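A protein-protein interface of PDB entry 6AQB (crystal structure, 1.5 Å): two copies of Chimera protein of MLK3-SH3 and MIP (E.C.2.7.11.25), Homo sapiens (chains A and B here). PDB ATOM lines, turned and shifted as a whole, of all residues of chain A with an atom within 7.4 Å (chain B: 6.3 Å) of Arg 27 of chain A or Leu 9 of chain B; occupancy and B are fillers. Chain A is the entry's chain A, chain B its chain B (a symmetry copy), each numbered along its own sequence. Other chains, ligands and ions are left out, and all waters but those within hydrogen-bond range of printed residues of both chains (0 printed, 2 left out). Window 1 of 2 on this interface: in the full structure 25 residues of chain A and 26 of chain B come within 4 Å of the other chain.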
ATOM      1  N   VAL A   5     -16.119  -5.171 -31.108  1.00  0.00           N
ATOM      2  CA  VAL A   5     -16.192  -5.018 -29.654  1.00  0.00           C
ATOM      3  C   VAL A   5     -16.485  -3.568 -29.334  1.00  0.00           C
ATOM      4  O   VAL A   5     -16.145  -2.668 -30.130  1.00  0.00           O
ATOM      5  CB  VAL A   5     -14.845  -5.508 -29.049  1.00  0.00           C
ATOM      6  CG1 VAL A   5     -14.829  -5.379 -27.568  1.00  0.00           C
ATOM      7  CG2 VAL A   5     -14.651  -6.999 -29.381  1.00  0.00           C
ATOM      8  N   TRP A   6     -17.162  -3.324 -28.189  1.00  0.00           N
ATOM      9  CA  TRP A   6     -17.363  -1.978 -27.657  1.00  0.00           C
ATOM     10  C   TRP A   6     -16.585  -1.853 -26.374  1.00  0.00           C
ATOM     11  O   TRP A   6     -16.500  -2.812 -25.547  1.00  0.00           O
ATOM     12  CB  TRP A   6     -18.815  -1.721 -27.367  1.00  0.00           C
ATOM     13  CG  TRP A   6     -19.699  -1.797 -28.578  1.00  0.00           C
ATOM     14  CD1 TRP A   6     -20.254  -2.921 -29.130  1.00  0.00           C
ATOM     15  CD2 TRP A   6     -20.128  -0.716 -29.344  1.00  0.00           C
ATOM     16  NE1 TRP A   6     -21.009  -2.583 -30.213  1.00  0.00           N
ATOM     17  CE2 TRP A   6     -20.935  -1.233 -30.382  1.00  0.00           C
ATOM     18  CE3 TRP A   6     -19.915   0.647 -29.270  1.00  0.00           C
ATOM     19  CZ2 TRP A   6     -21.531  -0.426 -31.317  1.00  0.00           C
ATOM     20  CZ3 TRP A   6     -20.495   1.455 -30.231  1.00  0.00           C
ATOM     21  CH2 TRP A   6     -21.287   0.912 -31.236  1.00  0.00           C
ATOM     22  N   THR A   7     -15.958  -0.671 -26.235  1.00  0.00           N
ATOM     23  CA  THR A   7     -15.120  -0.340 -25.097  1.00  0.00           C
ATOM     24  C   THR A   7     -15.647   0.924 -24.469  1.00  0.00           C
ATOM     25  O   THR A   7     -15.945   1.926 -25.180  1.00  0.00           O
ATOM     26  CB  THR A   7     -13.672  -0.131 -25.566  1.00  0.00           C
ATOM     27  OG1 THR A   7     -13.257  -1.322 -26.236  1.00  0.00           O
ATOM     28  CG2 THR A   7     -12.694   0.235 -24.465  1.00  0.00           C
ATOM     29  N   ALA A   8     -15.715   0.937 -23.140  1.00  0.00           N
ATOM     30  CA  ALA A   8     -15.984   2.176 -22.468  1.00  0.00           C
ATOM     31  C   ALA A   8     -14.792   3.182 -22.580  1.00  0.00           C
ATOM     32  O   ALA A   8     -13.665   2.830 -22.249  1.00  0.00           O
ATOM     33  CB  ALA A   8     -16.242   1.890 -21.015  1.00  0.00           C
ATOM     34  N   LEU A   9     -15.123   4.367 -22.968  1.00  0.00           N
ATOM     35  CA  LEU A   9     -14.111   5.415 -23.093  1.00  0.00           C
ATOM     36  C   LEU A   9     -14.072   6.313 -21.928  1.00  0.00           C
ATOM     37  O   LEU A   9     -13.170   7.168 -21.813  1.00  0.00           O
ATOM     38  CB  LEU A   9     -14.356   6.217 -24.351  1.00  0.00           C
ATOM     39  CG  LEU A   9     -14.067   5.534 -25.686  1.00  0.00           C
ATOM     40  CD1 LEU A   9     -14.444   6.540 -26.760  1.00  0.00           C
ATOM     41  CD2 LEU A   9     -12.619   5.156 -25.826  1.00  0.00           C
ATOM     42  N   LEU A  22     -19.558   1.678 -15.531  1.00  0.00           N
ATOM     43  CA  LEU A  22     -18.489   1.473 -16.551  1.00  0.00           C
ATOM     44  C   LEU A  22     -17.250   2.039 -15.952  1.00  0.00           C
ATOM     45  O   LEU A  22     -17.213   3.059 -15.309  1.00  0.00           O
ATOM     46  CB  LEU A  22     -18.816   2.183 -17.847  1.00  0.00           C
ATOM     47  CG  LEU A  22     -20.155   1.757 -18.475  1.00  0.00           C
ATOM     48  CD1 LEU A  22     -20.374   2.659 -19.690  1.00  0.00           C
ATOM     49  CD2 LEU A  22     -20.276   0.339 -18.786  1.00  0.00           C
ATOM     50  N   ARG A  23     -16.098   1.438 -16.364  1.00  0.00           N
ATOM     51  CA  ARG A  23     -14.782   1.987 -16.123  1.00  0.00           C
ATOM     52  C   ARG A  23     -14.040   2.084 -17.473  1.00  0.00           C
ATOM     53  O   ARG A  23     -14.155   1.155 -18.275  1.00  0.00           O
ATOM     54  CB  ARG A  23     -13.998   1.102 -15.133  1.00  0.00           C
ATOM     55  CG  ARG A  23     -14.539   1.129 -13.705  1.00  0.00           C
ATOM     56  CD  ARG A  23     -14.339   2.479 -12.975  1.00  0.00           C
ATOM     57  NE  ARG A  23     -12.964   2.616 -12.869  1.00  0.00           N
ATOM     58  CZ  ARG A  23     -12.154   2.030 -11.993  1.00  0.00           C
ATOM     59  NH1 ARG A  23     -12.595   1.319 -10.984  1.00  0.00           N
ATOM     60  NH2 ARG A  23     -10.819   2.090 -12.210  1.00  0.00           N
ATOM     61  N   LYS A  24     -13.291   3.148 -17.677  1.00  0.00           N
ATOM     62  CA  LYS A  24     -12.641   3.347 -18.952  1.00  0.00           C
ATOM     63  C   LYS A  24     -11.763   2.122 -19.275  1.00  0.00           C
ATOM     64  O   LYS A  24     -11.056   1.639 -18.444  1.00  0.00           O
ATOM     65  CB  LYS A  24     -11.682   4.498 -18.847  1.00  0.00           C
ATOM     66  CG  LYS A  24     -12.261   5.798 -18.473  1.00  0.00           C
ATOM     67  CD  LYS A  24     -11.188   6.718 -17.879  1.00  0.00           C
ATOM     68  CE  LYS A  24      -9.947   6.725 -18.708  1.00  0.00           C
ATOM     69  NZ  LYS A  24     -10.196   6.646 -20.175  1.00  0.00           N
ATOM     70  N   GLY A  25     -11.858   1.662 -20.493  1.00  0.00           N
ATOM     71  CA  GLY A  25     -11.137   0.494 -20.925  1.00  0.00           C
ATOM     72  C   GLY A  25     -11.898  -0.796 -20.780  1.00  0.00           C
ATOM     73  O   GLY A  25     -11.511  -1.765 -21.392  1.00  0.00           O
ATOM     74  N   ASP A  26     -13.092  -0.777 -20.100  1.00  0.00           N
ATOM     75  CA  ASP A  26     -13.863  -1.983 -20.025  1.00  0.00           C
ATOM     76  C   ASP A  26     -14.385  -2.398 -21.378  1.00  0.00           C
ATOM     77  O   ASP A  26     -14.861  -1.523 -22.107  1.00  0.00           O
ATOM     78  CB  ASP A  26     -15.159  -1.767 -19.231  1.00  0.00           C
ATOM     79  CG  ASP A  26     -14.980  -1.742 -17.754  1.00  0.00           C
ATOM     80  OD1 ASP A  26     -13.920  -2.087 -17.192  1.00  0.00           O
ATOM     81  OD2 ASP A  26     -15.951  -1.258 -17.062  1.00  0.00           O
ATOM     82  N   ARG A  27     -14.376  -3.665 -21.661  1.00  0.00           N
ATOM     83  CA  ARG A  27     -15.152  -4.175 -22.805  1.00  0.00           C
ATOM     84  C   ARG A  27     -16.578  -4.327 -22.319  1.00  0.00           C
ATOM     85  O   ARG A  27     -16.803  -4.791 -21.209  1.00  0.00           O
ATOM     86  CB  ARG A  27     -14.602  -5.505 -23.247  1.00  0.00           C
ATOM     87  CG  ARG A  27     -13.143  -5.413 -23.700  1.00  0.00           C
ATOM     88  CD  ARG A  27     -12.859  -4.382 -24.778  1.00  0.00           C
ATOM     89  NE  ARG A  27     -11.494  -4.719 -25.346  1.00  0.00           N
ATOM     90  CZ  ARG A  27     -10.559  -3.828 -25.704  1.00  0.00           C
ATOM     91  NH1 ARG A  27     -10.778  -2.542 -25.600  1.00  0.00           N
ATOM     92  NH2 ARG A  27      -9.373  -4.242 -26.188  1.00  0.00           N
ATOM     93  N   VAL A  28     -17.494  -3.862 -23.135  1.00  0.00           N
ATOM     94  CA  VAL A  28     -18.902  -3.880 -22.800  1.00  0.00           C
ATOM     95  C   VAL A  28     -19.564  -4.766 -23.841  1.00  0.00           C
ATOM     96  O   VAL A  28     -19.467  -4.497 -25.045  1.00  0.00           O
ATOM     97  CB  VAL A  28     -19.472  -2.482 -22.911  1.00  0.00           C
ATOM     98  CG1 VAL A  28     -20.984  -2.511 -22.596  1.00  0.00           C
ATOM     99  CG2 VAL A  28     -18.778  -1.548 -21.968  1.00  0.00           C
ATOM    100  N   GLU A  29     -20.234  -5.813 -23.394  1.00  0.00           N
ATOM    101  CA  GLU A  29     -20.978  -6.689 -24.287  1.00  0.00           C
ATOM    102  C   GLU A  29     -22.315  -6.058 -24.461  1.00  0.00           C
ATOM    103  O   GLU A  29     -22.998  -5.829 -23.493  1.00  0.00           O
ATOM    104  CB  GLU A  29     -21.086  -8.094 -23.663  1.00  0.00           C
ATOM    105  CG  GLU A  29     -22.007  -9.013 -24.402  1.00  0.00           C
ATOM    106  CD  GLU A  29     -21.932 -10.427 -23.875  1.00  0.00           C
ATOM    107  OE1 GLU A  29     -21.994 -10.607 -22.624  1.00  0.00           O
ATOM    108  OE2 GLU A  29     -21.823 -11.350 -24.721  1.00  0.00           O
ATOM    109  N   VAL A  30     -22.673  -5.642 -25.691  1.00  0.00           N
ATOM    110  CA  VAL A  30     -23.883  -4.932 -25.943  1.00  0.00           C
ATOM    111  C   VAL A  30     -24.971  -5.958 -26.269  1.00  0.00           C
ATOM    112  O   VAL A  30     -24.793  -6.732 -27.173  1.00  0.00           O
ATOM    113  CB  VAL A  30     -23.739  -3.921 -27.076  1.00  0.00           C
ATOM    114  CG1 VAL A  30     -25.076  -3.294 -27.388  1.00  0.00           C
ATOM    115  CG2 VAL A  30     -22.705  -2.841 -26.703  1.00  0.00           C
ATOM    116  N   GLN A  47     -23.679  -6.006 -20.788  1.00  0.00           N
ATOM    117  CA  GLN A  47     -23.115  -6.793 -19.714  1.00  0.00           C
ATOM    118  C   GLN A  47     -21.662  -6.416 -19.468  1.00  0.00           C
ATOM    119  O   GLN A  47     -20.855  -6.418 -20.405  1.00  0.00           O
ATOM    120  CB  GLN A  47     -23.236  -8.298 -19.986  1.00  0.00           C
ATOM    121  CG  GLN A  47     -22.565  -9.197 -18.942  1.00  0.00           C
ATOM    122  CD  GLN A  47     -21.070  -9.470 -19.098  1.00  0.00           C
ATOM    123  OE1 GLN A  47     -20.306  -9.278 -18.128  1.00  0.00           O
ATOM    124  NE2 GLN A  47     -20.635  -9.996 -20.262  1.00  0.00           N
ATOM    125  N   VAL A  48     -21.369  -6.206 -18.194  1.00  0.00           N
ATOM    126  CA  VAL A  48     -20.004  -6.018 -17.744  1.00  0.00           C
ATOM    127  C   VAL A  48     -19.810  -6.817 -16.454  1.00  0.00           C
ATOM    128  O   VAL A  48     -20.584  -6.684 -15.524  1.00  0.00           O
ATOM    129  CB  VAL A  48     -19.712  -4.561 -17.522  1.00  0.00           C
ATOM    130  CG1 VAL A  48     -18.332  -4.407 -16.897  1.00  0.00           C
ATOM    131  CG2 VAL A  48     -19.749  -3.793 -18.839  1.00  0.00           C
ATOM    132  N   GLY A  49     -18.733  -7.579 -16.353  1.00  0.00           N
ATOM    133  CA  GLY A  49     -18.420  -8.173 -15.022  1.00  0.00           C
ATOM    134  C   GLY A  49     -19.469  -9.082 -14.461  1.00  0.00           C
ATOM    135  O   GLY A  49     -19.597  -9.210 -13.254  1.00  0.00           O
ATOM    136  N   VAL A  60     -19.425   4.566 -24.865  1.00  0.00           N
ATOM    137  CA  VAL A  60     -18.716   3.490 -25.483  1.00  0.00           C
ATOM    138  C   VAL A  60     -18.373   3.807 -26.946  1.00  0.00           C
ATOM    139  O   VAL A  60     -19.025   4.648 -27.545  1.00  0.00           O
ATOM    140  CB  VAL A  60     -19.470   2.166 -25.396  1.00  0.00           C
ATOM    141  CG1 VAL A  60     -19.647   1.817 -23.936  1.00  0.00           C
ATOM    142  CG2 VAL A  60     -20.837   2.264 -26.124  1.00  0.00           C
ATOM    143  N   SER A  61     -17.358   3.109 -27.453  1.00  0.00           N
ATOM    144  CA  SER A  61     -16.902   3.212 -28.832  1.00  0.00           C
ATOM    145  C   SER A  61     -16.653   1.810 -29.388  1.00  0.00           C
ATOM    146  O   SER A  61     -16.192   0.899 -28.667  1.00  0.00           O
ATOM    147  CB  SER A  61     -15.614   3.987 -28.880  1.00  0.00           C
ATOM    148  OG  SER A  61     -15.525   4.638 -30.125  1.00  0.00           O
ATOM    149  N   ARG A  62     -16.982   1.652 -30.675  1.00  0.00           N
ATOM    150  CA  ARG A  62     -16.878   0.370 -31.378  1.00  0.00           C
ATOM    151  C   ARG A  62     -15.412   0.224 -31.765  1.00  0.00           C
ATOM    152  O   ARG A  62     -14.843   1.150 -32.349  1.00  0.00           O
ATOM    153  CB  ARG A  62     -17.758   0.413 -32.634  1.00  0.00           C
ATOM    154  CG  ARG A  62     -18.626  -0.778 -32.852  1.00  0.00           C
ATOM    155  CD  ARG A  62     -18.041  -1.815 -33.778  1.00  0.00           C
ATOM    156  NE  ARG A  62     -19.084  -2.793 -34.100  1.00  0.00           N
ATOM    157  CZ  ARG A  62     -19.540  -3.752 -33.283  1.00  0.00           C
ATOM    158  NH1 ARG A  62     -19.057  -3.917 -32.049  1.00  0.00           N
ATOM    159  NH2 ARG A  62     -20.500  -4.577 -33.708  1.00  0.00           N
ATOM    160  N   GLY A  63     -14.785  -0.889 -31.387  1.00  0.00           N
ATOM    161  CA  GLY A  63     -13.317  -0.954 -31.248  1.00  0.00           C
ATOM    162  C   GLY A  63     -12.867  -1.579 -29.931  1.00  0.00           C
ATOM    163  O   GLY A  63     -13.603  -1.539 -28.861  1.00  0.00           O
ATOM    164  N   GLY A  64     -11.654  -2.150 -29.996  1.00  0.00           N
ATOM    165  CA  GLY A  64     -11.399  -3.433 -29.322  1.00  0.00           C
ATOM    166  C   GLY A  64     -11.328  -4.655 -30.260  1.00  0.00           C
ATOM    167  O   GLY A  64     -11.290  -4.534 -31.474  1.00  0.00           O
ATOM    168  N   GLY A  65     -11.363  -5.842 -29.677  1.00  0.00           N
ATOM    169  CA  GLY A  65     -11.244  -7.098 -30.433  1.00  0.00           C
ATOM    170  C   GLY A  65      -9.800  -7.463 -30.234  1.00  0.00           C
ATOM    171  O   GLY A  65      -9.259  -7.378 -29.129  1.00  0.00           O
ATOM    172  N   ALA A  66      -9.124  -7.783 -31.312  1.00  0.00           N
ATOM    173  CA  ALA A  66      -7.773  -8.221 -31.171  1.00  0.00           C
ATOM    174  C   ALA A  66      -6.848  -7.015 -31.216  1.00  0.00           C
ATOM    175  O   ALA A  66      -7.091  -6.111 -32.021  1.00  0.00           O
ATOM    176  CB  ALA A  66      -7.410  -9.189 -32.293  1.00  0.00           C
ATOM    177  N   PRO A  67      -5.777  -7.078 -30.436  1.00  0.00           N
ATOM    178  CA  PRO A  67      -4.785  -6.034 -30.508  1.00  0.00           C
ATOM    179  C   PRO A  67      -4.196  -5.987 -31.914  1.00  0.00           C
ATOM    180  O   PRO A  67      -4.008  -7.061 -32.555  1.00  0.00           O
ATOM    181  CB  PRO A  67      -3.753  -6.384 -29.456  1.00  0.00           C
ATOM    182  CG  PRO A  67      -4.029  -7.777 -29.056  1.00  0.00           C
ATOM    183  CD  PRO A  67      -5.414  -8.090 -29.441  1.00  0.00           C
ATOM    184  N   PRO A  68      -3.955  -4.798 -32.449  1.00  0.00           N
ATOM    185  CA  PRO A  68      -3.451  -4.596 -33.794  1.00  0.00           C
ATOM    186  C   PRO A  68      -2.035  -5.134 -33.917  1.00  0.00           C
ATOM    187  O   PRO A  68      -1.287  -5.316 -32.947  1.00  0.00           O
ATOM    188  CB  PRO A  68      -3.445  -3.061 -33.926  1.00  0.00           C
ATOM    189  CG  PRO A  68      -4.398  -2.579 -32.953  1.00  0.00           C
ATOM    190  CD  PRO A  68      -4.384  -3.500 -31.861  1.00  0.00           C
ATOM    191  N   THR B   7      -6.739   7.684 -25.864  1.00  0.00           N
ATOM    192  CA  THR B   7      -6.974   6.575 -24.919  1.00  0.00           C
ATOM    193  C   THR B   7      -6.454   5.262 -25.566  1.00  0.00           C
ATOM    194  O   THR B   7      -6.744   4.994 -26.716  1.00  0.00           O
ATOM    195  CB  THR B   7      -8.478   6.455 -24.588  1.00  0.00           C
ATOM    196  OG1 THR B   7      -8.914   7.727 -24.025  1.00  0.00           O
ATOM    197  CG2 THR B   7      -8.792   5.334 -23.625  1.00  0.00           C
ATOM    198  N   ALA B   8      -5.749   4.483 -24.778  1.00  0.00           N
ATOM    199  CA  ALA B   8      -5.322   3.159 -25.195  1.00  0.00           C
ATOM    200  C   ALA B   8      -6.547   2.243 -25.273  1.00  0.00           C
ATOM    201  O   ALA B   8      -7.290   2.094 -24.332  1.00  0.00           O
ATOM    202  CB  ALA B   8      -4.303   2.546 -24.219  1.00  0.00           C
ATOM    203  N   LEU B   9      -6.711   1.633 -26.425  1.00  0.00           N
ATOM    204  CA  LEU B   9      -7.830   0.702 -26.632  1.00  0.00           C
ATOM    205  C   LEU B   9      -7.434  -0.779 -26.478  1.00  0.00           C
ATOM    206  O   LEU B   9      -8.301  -1.652 -26.424  1.00  0.00           O
ATOM    207  CB  LEU B   9      -8.416   0.904 -28.034  1.00  0.00           C
ATOM    208  CG  LEU B   9      -9.216   2.126 -28.367  1.00  0.00           C
ATOM    209  CD1 LEU B   9      -9.789   1.819 -29.775  1.00  0.00           C
ATOM    210  CD2 LEU B   9     -10.247   2.325 -27.312  1.00  0.00           C
ATOM    211  N   PHE B  10      -6.119  -1.018 -26.317  1.00  0.00           N
ATOM    212  CA  PHE B  10      -5.533  -2.332 -26.178  1.00  0.00           C
ATOM    213  C   PHE B  10      -4.350  -2.267 -25.254  1.00  0.00           C
ATOM    214  O   PHE B  10      -3.727  -1.219 -25.153  1.00  0.00           O
ATOM    215  CB  PHE B  10      -5.076  -2.945 -27.514  1.00  0.00           C
ATOM    216  CG  PHE B  10      -6.068  -2.876 -28.582  1.00  0.00           C
ATOM    217  CD1 PHE B  10      -6.981  -3.868 -28.749  1.00  0.00           C
ATOM    218  CD2 PHE B  10      -6.165  -1.768 -29.361  1.00  0.00           C
ATOM    219  CE1 PHE B  10      -7.928  -3.761 -29.750  1.00  0.00           C
ATOM    220  CE2 PHE B  10      -7.064  -1.693 -30.397  1.00  0.00           C
ATOM    221  CZ  PHE B  10      -7.954  -2.679 -30.566  1.00  0.00           C
ATOM    222  N   ASP B  11      -4.025  -3.380 -24.663  1.00  0.00           N
ATOM    223  CA  ASP B  11      -2.852  -3.517 -23.846  1.00  0.00           C
ATOM    224  C   ASP B  11      -1.682  -3.648 -24.848  1.00  0.00           C
ATOM    225  O   ASP B  11      -1.844  -4.272 -25.896  1.00  0.00           O
ATOM    226  CB  ASP B  11      -2.873  -4.791 -23.002  1.00  0.00           C
ATOM    227  CG  ASP B  11      -3.901  -4.791 -21.841  1.00  0.00           C
ATOM    228  OD1 ASP B  11      -4.514  -3.760 -21.517  1.00  0.00           O
ATOM    229  OD2 ASP B  11      -4.180  -5.919 -21.331  1.00  0.00           O
ATOM    230  N   ARG B  23      -2.056   0.057 -21.193  1.00  0.00           N
ATOM    231  CA  ARG B  23      -3.180  -0.866 -20.740  1.00  0.00           C
ATOM    232  C   ARG B  23      -4.468  -0.241 -21.168  1.00  0.00           C
ATOM    233  O   ARG B  23      -4.600   1.006 -21.130  1.00  0.00           O
ATOM    234  CB  ARG B  23      -3.144  -1.110 -19.263  1.00  0.00           C
ATOM    235  CG  ARG B  23      -1.846  -1.756 -18.760  1.00  0.00           C
ATOM    236  CD  ARG B  23      -1.738  -3.162 -19.166  1.00  0.00           C
ATOM    237  NE  ARG B  23      -0.506  -3.801 -18.642  1.00  0.00           N
ATOM    238  CZ  ARG B  23       0.645  -3.933 -19.330  1.00  0.00           C
ATOM    239  NH1 ARG B  23       0.778  -3.401 -20.511  1.00  0.00           N
ATOM    240  NH2 ARG B  23       1.680  -4.490 -18.761  1.00  0.00           N
ATOM    241  N   LYS B  24      -5.437  -1.082 -21.511  1.00  0.00           N
ATOM    242  CA  LYS B  24      -6.723  -0.564 -21.940  1.00  0.00           C
ATOM    243  C   LYS B  24      -7.313   0.473 -20.976  1.00  0.00           C
ATOM    244  O   LYS B  24      -7.352   0.288 -19.788  1.00  0.00           O
ATOM    245  CB  LYS B  24      -7.802  -1.611 -22.001  1.00  0.00           C
ATOM    246  CG  LYS B  24      -7.628  -2.601 -23.064  1.00  0.00           C
ATOM    247  CD  LYS B  24      -8.629  -3.769 -22.742  1.00  0.00           C
ATOM    248  CE  LYS B  24      -8.042  -4.587 -21.635  1.00  0.00           C
ATOM    249  NZ  LYS B  24      -8.889  -5.588 -20.982  1.00  0.00           N
ATOM    250  N   GLY B  25      -7.742   1.551 -21.623  1.00  0.00           N
ATOM    251  CA  GLY B  25      -8.283   2.702 -20.899  1.00  0.00           C
ATOM    252  C   GLY B  25      -7.275   3.748 -20.434  1.00  0.00           C
ATOM    253  O   GLY B  25      -7.670   4.813 -19.942  1.00  0.00           O
ATOM    254  N   ASP B  26      -5.963   3.491 -20.541  1.00  0.00           N
ATOM    255  CA  ASP B  26      -4.980   4.491 -20.191  1.00  0.00           C
ATOM    256  C   ASP B  26      -5.178   5.769 -21.001  1.00  0.00           C
ATOM    257  O   ASP B  26      -5.441   5.740 -22.214  1.00  0.00           O
ATOM    258  CB  ASP B  26      -3.596   4.039 -20.592  1.00  0.00           C
ATOM    259  CG  ASP B  26      -2.925   3.158 -19.640  1.00  0.00           C
ATOM    260  OD1 ASP B  26      -3.341   2.913 -18.490  1.00  0.00           O
ATOM    261  OD2 ASP B  26      -1.916   2.530 -20.111  1.00  0.00           O
ATOM    262  N   ASN B  58      -1.403   2.682 -33.647  1.00  0.00           N
ATOM    263  CA  ASN B  58      -2.655   2.037 -33.851  1.00  0.00           C
ATOM    264  C   ASN B  58      -3.278   1.423 -32.606  1.00  0.00           C
ATOM    265  O   ASN B  58      -4.372   0.882 -32.692  1.00  0.00           O
ATOM    266  CB  ASN B  58      -2.521   1.005 -35.009  1.00  0.00           C
ATOM    267  CG  ASN B  58      -1.428  -0.040 -34.797  1.00  0.00           C
ATOM    268  OD1 ASN B  58      -0.591  -0.014 -33.894  1.00  0.00           O
ATOM    269  ND2 ASN B  58      -1.383  -0.997 -35.755  1.00  0.00           N
ATOM    270  N   TYR B  59      -2.678   1.593 -31.443  1.00  0.00           N
ATOM    271  CA  TYR B  59      -3.210   1.100 -30.168  1.00  0.00           C
ATOM    272  C   TYR B  59      -4.062   2.178 -29.411  1.00  0.00           C
ATOM    273  O   TYR B  59      -4.653   1.830 -28.394  1.00  0.00           O
ATOM    274  CB  TYR B  59      -2.116   0.571 -29.282  1.00  0.00           C
ATOM    275  CG  TYR B  59      -1.684  -0.815 -29.586  1.00  0.00           C
ATOM    276  CD1 TYR B  59      -1.247  -1.170 -30.867  1.00  0.00           C
ATOM    277  CD2 TYR B  59      -1.750  -1.806 -28.650  1.00  0.00           C
ATOM    278  CE1 TYR B  59      -0.904  -2.489 -31.144  1.00  0.00           C
ATOM    279  CE2 TYR B  59      -1.420  -3.123 -28.932  1.00  0.00           C
ATOM    280  CZ  TYR B  59      -0.976  -3.444 -30.156  1.00  0.00           C
ATOM    281  OH  TYR B  59      -0.691  -4.773 -30.379  1.00  0.00           O
ATOM    282  N   VAL B  60      -4.116   3.386 -29.944  1.00  0.00           N
ATOM    283  CA  VAL B  60      -4.829   4.458 -29.275  1.00  0.00           C
ATOM    284  C   VAL B  60      -5.919   5.046 -30.216  1.00  0.00           C
ATOM    285  O   VAL B  60      -5.835   4.992 -31.465  1.00  0.00           O
ATOM    286  CB  VAL B  60      -3.875   5.597 -28.837  1.00  0.00           C
ATOM    287  CG1 VAL B  60      -2.946   5.059 -27.775  1.00  0.00           C
ATOM    288  CG2 VAL B  60      -3.138   6.126 -30.011  1.00  0.00           C
ATOM    289  N   SER B  61      -6.883   5.644 -29.565  1.00  0.00           N
ATOM    290  CA  SER B  61      -8.031   6.264 -30.241  1.00  0.00           C
ATOM    291  C   SER B  61      -8.161   7.701 -29.665  1.00  0.00           C
ATOM    292  O   SER B  61      -7.964   7.907 -28.464  1.00  0.00           O
ATOM    293  CB  SER B  61      -9.280   5.419 -29.977  1.00  0.00           C
ATOM    294  OG  SER B  61     -10.404   5.866 -30.720  1.00  0.00           O
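The side-chain amino group (NZ) of Lys 24 of chain A is in hydrogen-bond range of the backbone carbonyl oxygen (O) of Gly 25 of chain B, 3.1 Å away. The guanidinium group (NH1) of Arg 27 of chain A sits at hydrogen-bond distance from the backbone carbonyl oxygen (O) of Leu 9 of chain B (2.8 Å). The backbone carbonyl oxygen of Pro 68 of chain A sits at hydrogen-bond distance from the side-chain hydroxyl of Tyr 59 of chain B (2.7 Å).
The side-chain hydroxyl (OG1) of Thr 7 of chain A is in hydrogen-bond range of the guanidinium group (NH1) of Arg 27 of chain A, 2.8 Å away. O of Ala 8 of chain A sits at hydrogen-bond distance from N of Gly 25 of chain A, 2.8 Å away. The backbone carbonyl oxygen (O) of Leu 9 of chain A lies within hydrogen-bond range of the side-chain amino group (NZ) of Lys 24 of chain A, 3.4 Å away. The backbone NH of Thr 7 of chain B is in hydrogen-bond range of the backbone carbonyl oxygen of Ser 61 of chain B. N of Leu 9 of chain B lies within hydrogen-bond range of O of Tyr 59 of chain B, at 2.9 Å. The side-chain carboxylate (OD1) of Asp 11 of chain B sits at hydrogen-bond distance from the backbone NH (N) of Lys 24 of chain B (2.8 Å).
Leu 9 of chain A touches Leu 9 of chain B (CD2 to CD2, 3.98 Å). CG2 of Thr 7 of chain B touches NZ of Lys 24 of chain A, at 3.9 Å. CD of Lys 24 of chain B touches O of Gly 25 of chain A (3.8 Å). Gly 25 of chain A touches Gly 25 of chain B (CA to CA, 3.6 Å). Arg 27 of chain A touches Phe 10 of chain B. Phe 10 of chain B touches Gly 64 of chain A (CE1 to CA, 3.5 Å). Ala 66 of chain A touches Phe 10 of chain B. CA of Pro 67 of chain A touches CD1 of Phe 10 of chain B, 3.6 Å away. Pro 67 of chain A touches Tyr 59 of chain B (CB to OH, 3.6 Å). CD of Pro 68 of chain A touches CD2 of Phe 10 of chain B (3.5 Å).
Val 5 of chain A touches none of the printed residues of chain B. Printed residues of chain B within 4 Å of Lys 24 of chain A: Thr 7 and Gly 25. Of chain B, only Leu 9, Phe 10 and Lys 24 come within 4 Å of Arg 27 of chain A. Printed residues of chain A within 4 Å of Leu 9 of chain B: Leu 9 and Arg 27. Printed residues of chain A within 4 Å of Phe 10 of chain B: Arg 27 (3.5 Å), Gly 64 (3.5 Å), Gly 65 (3.9 Å), Ala 66 (3.4 Å), Pro 67 (3.6 Å) and Pro 68 (3.5 Å). Of the printed residues of chain A, Tyr 59 of chain B touches Pro 67 (3.6 Å) and Pro 68 (2.7 Å).
Printed residues of chain B that touch a printed residue of chain A: Thr 7, Leu 9, Phe 10, Lys 24, Gly 25, Asn 58 and Tyr 59. Of the 26 printed residues of chain A, 9 touch a printed residue of chain B. Among the printed residues, 16 pairs touch across the chains. Among the printed residues, no Asp or Glu carboxylate lies within 4 Å of a Lys or Arg side-chain nitrogen of the other chain.
Leu 9 of chain A touches its own counterpart, Leu 9 of chain B. Lys 24 of chain A touches Thr 7 of chain B, but with the chains exchanged Thr 7 of chain A does not touch Lys 24 of chain B (5.8 Å). Lys 24 of chain A touches Gly 25 of chain B, and with the chains exchanged Gly 25 of chain A touches Lys 24 of chain B. Gly 25 of chain A touches its own counterpart, Gly 25 of chain B. 9 positions are printed for both chains. Of the 16 pairs that touch across the chains among the printed residues, 4 have their exchanged pair printed and touching as well.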
